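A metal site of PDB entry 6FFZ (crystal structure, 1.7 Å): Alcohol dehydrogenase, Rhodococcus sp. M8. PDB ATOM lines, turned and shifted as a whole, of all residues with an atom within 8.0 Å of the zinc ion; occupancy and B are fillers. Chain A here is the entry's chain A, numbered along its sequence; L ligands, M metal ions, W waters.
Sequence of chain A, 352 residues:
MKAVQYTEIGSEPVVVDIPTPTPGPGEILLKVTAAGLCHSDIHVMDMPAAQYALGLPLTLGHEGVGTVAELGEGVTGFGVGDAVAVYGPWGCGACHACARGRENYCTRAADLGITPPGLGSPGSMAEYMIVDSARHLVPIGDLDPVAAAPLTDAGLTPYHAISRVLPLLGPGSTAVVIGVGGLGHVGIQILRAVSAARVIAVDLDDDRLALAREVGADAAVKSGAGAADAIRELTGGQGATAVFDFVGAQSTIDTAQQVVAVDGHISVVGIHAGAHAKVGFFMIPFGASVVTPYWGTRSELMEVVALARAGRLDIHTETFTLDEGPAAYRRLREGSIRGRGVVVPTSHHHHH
N of Ser 40 lies within hydrogen-bond range of O13 of the ligand. OG of Ser 40 lies within hydrogen-bond range of O13 of the ligand. The guanidinium group (NH1) of Arg 340 lies within salt-bridge range of an oxygen (O8) of the ligand (2.8 Å). N of His 39 lies within hydrogen-bond range of O8 of the ligand, at 3.1 Å. A ring nitrogen (ND1) of His 39 is in hydrogen-bond range of an oxygen (O1) of the ligand, at 2.8 Å. The backbone NH of Trp 295 lies within hydrogen-bond range of an oxygen (O14) of the ligand, at 2.9 Å. N of Leu 183 is in hydrogen-bond range of O9 of the ligand, at 2.9 Å. An oxygen (O12) of the ligand lies within hydrogen-bond range of the backbone NH (N) of Ile 271 (3.0 Å). An oxygen (O12) of the ligand sits at hydrogen-bond distance from the backbone carbonyl oxygen (O) of Ile 271, at 3.3 Å.
Residues that only touch the zinc ion: Ser 40. Within 4 Å of the zinc ion: Cys 38, Ser 40, His 62 and Asp 153.
The zinc ion is bound by OD2 of Asp 153 (1.9 Å), NE2 of His 62 (2.1 Å), water W1 (2.1 Å) and SG of Cys 38 (2.3 Å). The zinc ion has four donor atoms within binding distance.
The side-chain carboxylate (OD1) of Asp 153 lies within hydrogen-bond range of the side-chain hydroxyl (OG1) of Thr 157, at 2.7 Å. ND1 of His 62 sits close to OD1 of Asp 41, at 3.2 Å. The backbone NH (N) of Ser 40 lies close to the side-chain sulfur (SG) of Cys 38. NH2 of Arg 340 sits close to SG of Cys 38, at 3.4 Å. The backbone NH of Cys 38 sits at hydrogen-bond distance from the side-chain carboxylate of Asp 41 (3.2 Å).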
ATOM      1  N   GLY A  36      -8.023  -0.489  -1.346  1.00  0.00           N
ATOM      2  CA  GLY A  36      -8.462  -1.866  -1.176  1.00  0.00           C
ATOM      3  C   GLY A  36      -9.418  -2.322  -2.288  1.00  0.00           C
ATOM      4  O   GLY A  36     -10.234  -1.543  -2.762  1.00  0.00           O
ATOM      5  N   LEU A  37      -9.289  -3.586  -2.667  1.00  0.00           N
ATOM      6  CA  LEU A  37     -10.229  -4.263  -3.547  1.00  0.00           C
ATOM      7  C   LEU A  37     -11.251  -4.991  -2.701  1.00  0.00           C
ATOM      8  O   LEU A  37     -10.894  -5.625  -1.724  1.00  0.00           O
ATOM      9  CB  LEU A  37      -9.524  -5.321  -4.397  1.00  0.00           C
ATOM     10  CG  LEU A  37      -8.680  -4.888  -5.560  1.00  0.00           C
ATOM     11  CD1 LEU A  37      -7.336  -4.320  -5.136  1.00  0.00           C
ATOM     12  CD2 LEU A  37      -8.492  -6.102  -6.452  1.00  0.00           C
ATOM     13  N   CYS A  38     -12.522  -4.890  -3.070  1.00  0.00           N
ATOM     14  CA  CYS A  38     -13.605  -5.508  -2.297  1.00  0.00           C
ATOM     15  C   CYS A  38     -14.408  -6.396  -3.223  1.00  0.00           C
ATOM     16  O   CYS A  38     -14.589  -6.077  -4.392  1.00  0.00           O
ATOM     17  CB  CYS A  38     -14.522  -4.454  -1.712  1.00  0.00           C
ATOM     18  SG  CYS A  38     -15.896  -5.109  -0.760  1.00  0.00           S
ATOM     19  N   HIS A  39     -14.959  -7.504  -2.698  1.00  0.00           N
ATOM     20  CA  HIS A  39     -15.779  -8.385  -3.521  1.00  0.00           C
ATOM     21  C   HIS A  39     -17.006  -7.639  -4.052  1.00  0.00           C
ATOM     22  O   HIS A  39     -17.523  -7.996  -5.101  1.00  0.00           O
ATOM     23  CB  HIS A  39     -16.225  -9.612  -2.726  1.00  0.00           C
ATOM     24  CG  HIS A  39     -16.586 -10.795  -3.577  1.00  0.00           C
ATOM     25  ND1 HIS A  39     -15.770 -11.910  -3.664  1.00  0.00           N
ATOM     26  CD2 HIS A  39     -17.643 -11.029  -4.394  1.00  0.00           C
ATOM     27  CE1 HIS A  39     -16.316 -12.777  -4.503  1.00  0.00           C
ATOM     28  NE2 HIS A  39     -17.450 -12.265  -4.964  1.00  0.00           N
ATOM     29  N   SER A  40     -17.462  -6.577  -3.366  1.00  0.00           N
ATOM     30  CA  SER A  40     -18.536  -5.748  -3.908  1.00  0.00           C
ATOM     31  C   SER A  40     -18.210  -5.173  -5.297  1.00  0.00           C
ATOM     32  O   SER A  40     -19.125  -4.953  -6.087  1.00  0.00           O
ATOM     33  CB  SER A  40     -18.930  -4.618  -2.958  1.00  0.00           C
ATOM     34  OG  SER A  40     -19.560  -5.119  -1.822  1.00  0.00           O
ATOM     35  N   ASP A  41     -16.933  -4.927  -5.577  1.00  0.00           N
ATOM     36  CA  ASP A  41     -16.518  -4.455  -6.896  1.00  0.00           C
ATOM     37  C   ASP A  41     -16.812  -5.476  -7.979  1.00  0.00           C
ATOM     38  O   ASP A  41     -17.167  -5.123  -9.105  1.00  0.00           O
ATOM     39  CB  ASP A  41     -15.026  -4.115  -6.923  1.00  0.00           C
ATOM     40  CG  ASP A  41     -14.638  -3.030  -5.945  1.00  0.00           C
ATOM     41  OD1 ASP A  41     -15.510  -2.176  -5.646  1.00  0.00           O
ATOM     42  OD2 ASP A  41     -13.476  -3.001  -5.472  1.00  0.00           O
ATOM     43  N   GLY A  61     -12.557   1.677  -6.317  1.00  0.00           N
ATOM     44  CA  GLY A  61     -11.849   1.757  -5.049  1.00  0.00           C
ATOM     45  C   GLY A  61     -12.642   2.510  -4.024  1.00  0.00           C
ATOM     46  O   GLY A  61     -12.609   3.745  -3.978  1.00  0.00           O
ATOM     47  N   HIS A  62     -13.352   1.775  -3.178  1.00  0.00           N
ATOM     48  CA  HIS A  62     -14.107   2.406  -2.106  1.00  0.00           C
ATOM     49  C   HIS A  62     -13.478   2.169  -0.734  1.00  0.00           C
ATOM     50  O   HIS A  62     -14.070   2.529   0.299  1.00  0.00           O
ATOM     51  CB  HIS A  62     -15.580   1.992  -2.141  1.00  0.00           C
ATOM     52  CG  HIS A  62     -15.813   0.525  -2.048  1.00  0.00           C
ATOM     53  ND1 HIS A  62     -15.902  -0.281  -3.159  1.00  0.00           N
ATOM     54  CD2 HIS A  62     -16.033  -0.277  -0.974  1.00  0.00           C
ATOM     55  CE1 HIS A  62     -16.154  -1.527  -2.763  1.00  0.00           C
ATOM     56  NE2 HIS A  62     -16.241  -1.540  -1.450  1.00  0.00           N
ATOM     57  N   GLU A  63     -12.267   1.609  -0.737  1.00  0.00           N
ATOM     58  CA  GLU A  63     -11.426   1.477   0.445  1.00  0.00           C
ATOM     59  C   GLU A  63     -10.198   2.309   0.186  1.00  0.00           C
ATOM     60  O   GLU A  63      -9.343   1.902  -0.568  1.00  0.00           O
ATOM     61  CB  GLU A  63     -11.001   0.024   0.684  1.00  0.00           C
ATOM     62  CG  GLU A  63     -12.097  -0.884   1.229  1.00  0.00           C
ATOM     63  CD  GLU A  63     -11.598  -2.256   1.689  1.00  0.00           C
ATOM     64  OE1 GLU A  63     -10.507  -2.699   1.298  1.00  0.00           O
ATOM     65  OE2 GLU A  63     -12.305  -2.929   2.463  1.00  0.00           O
ATOM     66  N   LEU A 119     -18.035   3.901  -6.082  1.00  0.00           N
ATOM     67  CA  LEU A 119     -19.364   3.301  -6.235  1.00  0.00           C
ATOM     68  C   LEU A 119     -20.371   4.352  -6.717  1.00  0.00           C
ATOM     69  O   LEU A 119     -21.513   4.414  -6.256  1.00  0.00           O
ATOM     70  CB  LEU A 119     -19.796   2.664  -4.933  1.00  0.00           C
ATOM     71  CG  LEU A 119     -18.950   1.526  -4.389  1.00  0.00           C
ATOM     72  CD1 LEU A 119     -19.336   1.162  -2.974  1.00  0.00           C
ATOM     73  CD2 LEU A 119     -19.085   0.301  -5.289  1.00  0.00           C
ATOM     74  N   THR A 152     -11.422   0.671   6.180  1.00  0.00           N
ATOM     75  CA  THR A 152     -12.533   1.482   5.704  1.00  0.00           C
ATOM     76  C   THR A 152     -13.782   0.706   5.249  1.00  0.00           C
ATOM     77  O   THR A 152     -14.822   1.302   5.057  1.00  0.00           O
ATOM     78  CB  THR A 152     -12.091   2.403   4.549  1.00  0.00           C
ATOM     79  OG1 THR A 152     -11.606   1.614   3.463  1.00  0.00           O
ATOM     80  CG2 THR A 152     -11.003   3.341   5.003  1.00  0.00           C
ATOM     81  N   ASP A 153     -13.665  -0.604   5.073  1.00  0.00           N
ATOM     82  CA  ASP A 153     -14.829  -1.425   4.667  1.00  0.00           C
ATOM     83  C   ASP A 153     -14.693  -2.836   5.206  1.00  0.00           C
ATOM     84  O   ASP A 153     -15.541  -3.289   5.966  1.00  0.00           O
ATOM     85  CB  ASP A 153     -14.968  -1.356   3.152  1.00  0.00           C
ATOM     86  CG  ASP A 153     -16.219  -2.021   2.626  1.00  0.00           C
ATOM     87  OD1 ASP A 153     -17.183  -2.270   3.369  1.00  0.00           O
ATOM     88  OD2 ASP A 153     -16.221  -2.260   1.417  1.00  0.00           O
ATOM     89  N   ALA A 154     -13.602  -3.529   4.877  1.00  0.00           N
ATOM     90  CA  ALA A 154     -13.352  -4.847   5.511  1.00  0.00           C
ATOM     91  C   ALA A 154     -13.357  -4.763   7.024  1.00  0.00           C
ATOM     92  O   ALA A 154     -13.727  -5.711   7.675  1.00  0.00           O
ATOM     93  CB  ALA A 154     -12.058  -5.453   4.993  1.00  0.00           C
ATOM     94  N   THR A 157     -17.374  -2.521   8.016  1.00  0.00           N
ATOM     95  CA  THR A 157     -18.642  -3.220   7.794  1.00  0.00           C
ATOM     96  C   THR A 157     -18.859  -4.313   8.861  1.00  0.00           C
ATOM     97  O   THR A 157     -19.927  -4.338   9.485  1.00  0.00           O
ATOM     98  CB  THR A 157     -18.740  -3.713   6.359  1.00  0.00           C
ATOM     99  OG1 THR A 157     -18.762  -2.556   5.505  1.00  0.00           O
ATOM    100  CG2 THR A 157     -19.974  -4.535   6.144  1.00  0.00           C
ATOM    101  N   LEU A 183     -13.557  -9.339   4.668  1.00  0.00           N
ATOM    102  CA  LEU A 183     -14.355  -8.934   5.798  1.00  0.00           C
ATOM    103  C   LEU A 183     -14.239  -9.921   6.971  1.00  0.00           C
ATOM    104  O   LEU A 183     -14.000  -9.522   8.116  1.00  0.00           O
ATOM    105  CB  LEU A 183     -15.845  -8.787   5.417  1.00  0.00           C
ATOM    106  CG  LEU A 183     -16.272  -7.424   4.927  1.00  0.00           C
ATOM    107  CD1 LEU A 183     -15.625  -7.088   3.589  1.00  0.00           C
ATOM    108  CD2 LEU A 183     -17.781  -7.312   4.841  1.00  0.00           C
ATOM    109  N   ILE A 271     -23.399 -10.459   0.147  1.00  0.00           N
ATOM    110  CA  ILE A 271     -24.415 -10.201  -0.871  1.00  0.00           C
ATOM    111  C   ILE A 271     -24.367 -11.302  -1.927  1.00  0.00           C
ATOM    112  O   ILE A 271     -23.313 -11.558  -2.558  1.00  0.00           O
ATOM    113  CB  ILE A 271     -24.198  -8.805  -1.507  1.00  0.00           C
ATOM    114  CG1 ILE A 271     -24.230  -7.701  -0.432  1.00  0.00           C
ATOM    115  CG2 ILE A 271     -25.228  -8.534  -2.604  1.00  0.00           C
ATOM    116  CD1 ILE A 271     -23.596  -6.390  -0.869  1.00  0.00           C
ATOM    117  N   TYR A 294     -25.527  -2.274   6.440  1.00  0.00           N
ATOM    118  CA  TYR A 294     -24.818  -1.607   5.343  1.00  0.00           C
ATOM    119  C   TYR A 294     -23.687  -0.755   5.893  1.00  0.00           C
ATOM    120  O   TYR A 294     -23.925   0.187   6.643  1.00  0.00           O
ATOM    121  CB  TYR A 294     -25.760  -0.722   4.571  1.00  0.00           C
ATOM    122  CG  TYR A 294     -25.100   0.115   3.499  1.00  0.00           C
ATOM    123  CD1 TYR A 294     -24.364  -0.478   2.470  1.00  0.00           C
ATOM    124  CD2 TYR A 294     -25.208   1.475   3.512  1.00  0.00           C
ATOM    125  CE1 TYR A 294     -23.784   0.307   1.469  1.00  0.00           C
ATOM    126  CE2 TYR A 294     -24.639   2.279   2.513  1.00  0.00           C
ATOM    127  CZ  TYR A 294     -23.929   1.679   1.507  1.00  0.00           C
ATOM    128  OH  TYR A 294     -23.353   2.469   0.537  1.00  0.00           O
ATOM    129  N   TRP A 295     -22.477  -1.129   5.486  1.00  0.00           N
ATOM    130  CA  TRP A 295     -21.262  -0.372   5.754  1.00  0.00           C
ATOM    131  C   TRP A 295     -21.163  -0.004   7.230  1.00  0.00           C
ATOM    132  O   TRP A 295     -21.321  -0.886   8.055  1.00  0.00           O
ATOM    133  CB  TRP A 295     -21.167   0.797   4.753  1.00  0.00           C
ATOM    134  CG  TRP A 295     -19.785   1.069   4.267  1.00  0.00           C
ATOM    135  CD1 TRP A 295     -18.613   0.890   4.952  1.00  0.00           C
ATOM    136  CD2 TRP A 295     -19.434   1.581   2.996  1.00  0.00           C
ATOM    137  NE1 TRP A 295     -17.536   1.243   4.163  1.00  0.00           N
ATOM    138  CE2 TRP A 295     -18.017   1.675   2.961  1.00  0.00           C
ATOM    139  CE3 TRP A 295     -20.169   1.959   1.879  1.00  0.00           C
ATOM    140  CZ2 TRP A 295     -17.338   2.138   1.840  1.00  0.00           C
ATOM    141  CZ3 TRP A 295     -19.497   2.427   0.769  1.00  0.00           C
ATOM    142  CH2 TRP A 295     -18.096   2.508   0.766  1.00  0.00           C
ATOM    143  N   ARG A 340      -7.060  -9.371   2.102  1.00  0.00           N
ATOM    144  CA  ARG A 340      -7.443  -8.236   1.265  1.00  0.00           C
ATOM    145  C   ARG A 340      -6.395  -7.884   0.257  1.00  0.00           C
ATOM    146  O   ARG A 340      -5.210  -7.788   0.596  1.00  0.00           O
ATOM    147  CB  ARG A 340      -7.703  -7.003   2.156  1.00  0.00           C
ATOM    148  CG  ARG A 340      -9.152  -6.685   2.323  1.00  0.00           C
ATOM    149  CD  ARG A 340      -9.729  -6.073   1.093  1.00  0.00           C
ATOM    150  NE  ARG A 340     -11.043  -5.488   1.361  1.00  0.00           N
ATOM    151  CZ  ARG A 340     -12.235  -6.088   1.189  1.00  0.00           C
ATOM    152  NH1 ARG A 340     -12.330  -7.361   0.819  1.00  0.00           N
ATOM    153  NH2 ARG A 340     -13.325  -5.392   1.417  1.00  0.00           N
HETATM  154  P1  LIG L   1     -13.754 -12.157  -0.316  1.00  0.00           P
HETATM  155  O1  LIG L   1     -13.896 -12.574  -1.716  1.00  0.00           O
HETATM  156  O2  LIG L   1     -12.533 -11.480   0.285  1.00  0.00           O
HETATM  157  O3  LIG L   1     -13.991 -13.421   0.654  1.00  0.00           O
HETATM  158  C1  LIG L   1     -14.901 -14.484   0.338  1.00  0.00           C
HETATM  159  C2  LIG L   1     -14.685 -15.588   1.368  1.00  0.00           C
HETATM  160  O4  LIG L   1     -15.903 -16.298   1.503  1.00  0.00           O
HETATM  161  C3  LIG L   1     -13.618 -16.585   0.974  1.00  0.00           C
HETATM  162  O5  LIG L   1     -12.813 -16.872   2.122  1.00  0.00           O
HETATM  163  C4  LIG L   1     -14.415 -17.806   0.534  1.00  0.00           C
HETATM  164  O6  LIG L   1     -13.785 -19.063   0.654  1.00  0.00           O
HETATM  165  C5  LIG L   1     -15.647 -17.691   1.421  1.00  0.00           C
HETATM  166  N1  LIG L   1     -16.843 -18.394   0.958  1.00  0.00           N
HETATM  167  C6  LIG L   1     -17.396 -18.317  -0.271  1.00  0.00           C
HETATM  168  N2  LIG L   1     -18.505 -19.095  -0.341  1.00  0.00           N
HETATM  169  C7  LIG L   1     -18.682 -19.641   0.897  1.00  0.00           C
HETATM  170  C8  LIG L   1     -19.643 -20.552   1.505  1.00  0.00           C
HETATM  171  N3  LIG L   1     -20.690 -21.057   0.829  1.00  0.00           N
HETATM  172  N4  LIG L   1     -19.427 -20.880   2.800  1.00  0.00           N
HETATM  173  C9  LIG L   1     -18.388 -20.400   3.528  1.00  0.00           C
HETATM  174  N5  LIG L   1     -17.465 -19.575   3.017  1.00  0.00           N
HETATM  175  C10 LIG L   1     -17.568 -19.196   1.726  1.00  0.00           C
HETATM  176  O7  LIG L   1     -15.070 -11.280  -0.030  1.00  0.00           O
HETATM  177  P2  LIG L   1     -15.199  -9.926   0.864  1.00  0.00           P
HETATM  178  O8  LIG L   1     -14.578  -8.836   0.057  1.00  0.00           O
HETATM  179  O9  LIG L   1     -14.803 -10.268   2.267  1.00  0.00           O
HETATM  180  O10 LIG L   1     -16.788  -9.697   0.798  1.00  0.00           O
HETATM  181  C11 LIG L   1     -17.679 -10.661   1.376  1.00  0.00           C
HETATM  182  C12 LIG L   1     -19.099 -10.278   1.005  1.00  0.00           C
HETATM  183  O11 LIG L   1     -19.479  -9.147   1.791  1.00  0.00           O
HETATM  184  C13 LIG L   1     -19.352  -9.955  -0.468  1.00  0.00           C
HETATM  185  O12 LIG L   1     -20.622 -10.495  -0.892  1.00  0.00           O
HETATM  186  C14 LIG L   1     -19.385  -8.442  -0.476  1.00  0.00           C
HETATM  187  O13 LIG L   1     -20.084  -7.829  -1.570  1.00  0.00           O
HETATM  188  C15 LIG L   1     -20.074  -8.197   0.873  1.00  0.00           C
HETATM  189  N6  LIG L   1     -19.970  -6.876   1.463  1.00  0.00           N
HETATM  190  C16 LIG L   1     -21.071  -6.323   1.996  1.00  0.00           C
HETATM  191  C17 LIG L   1     -21.035  -5.086   2.617  1.00  0.00           C
HETATM  192  C18 LIG L   1     -22.265  -4.518   3.267  1.00  0.00           C
HETATM  193  O14 LIG L   1     -22.268  -3.335   3.550  1.00  0.00           O
HETATM  194  N7  LIG L   1     -23.306  -5.284   3.672  1.00  0.00           N
HETATM  195  C19 LIG L   1     -19.812  -4.343   2.652  1.00  0.00           C
HETATM  196  C20 LIG L   1     -18.657  -4.963   2.112  1.00  0.00           C
HETATM  197  C21 LIG L   1     -18.769  -6.212   1.502  1.00  0.00           C
HETATM  198 ZN    ZN M   1     -16.802  -3.066  -0.174  1.00  0.00          ZN
HETATM  199  O   HOH W   1     -18.870  -2.923  -0.297  1.00  0.00           O
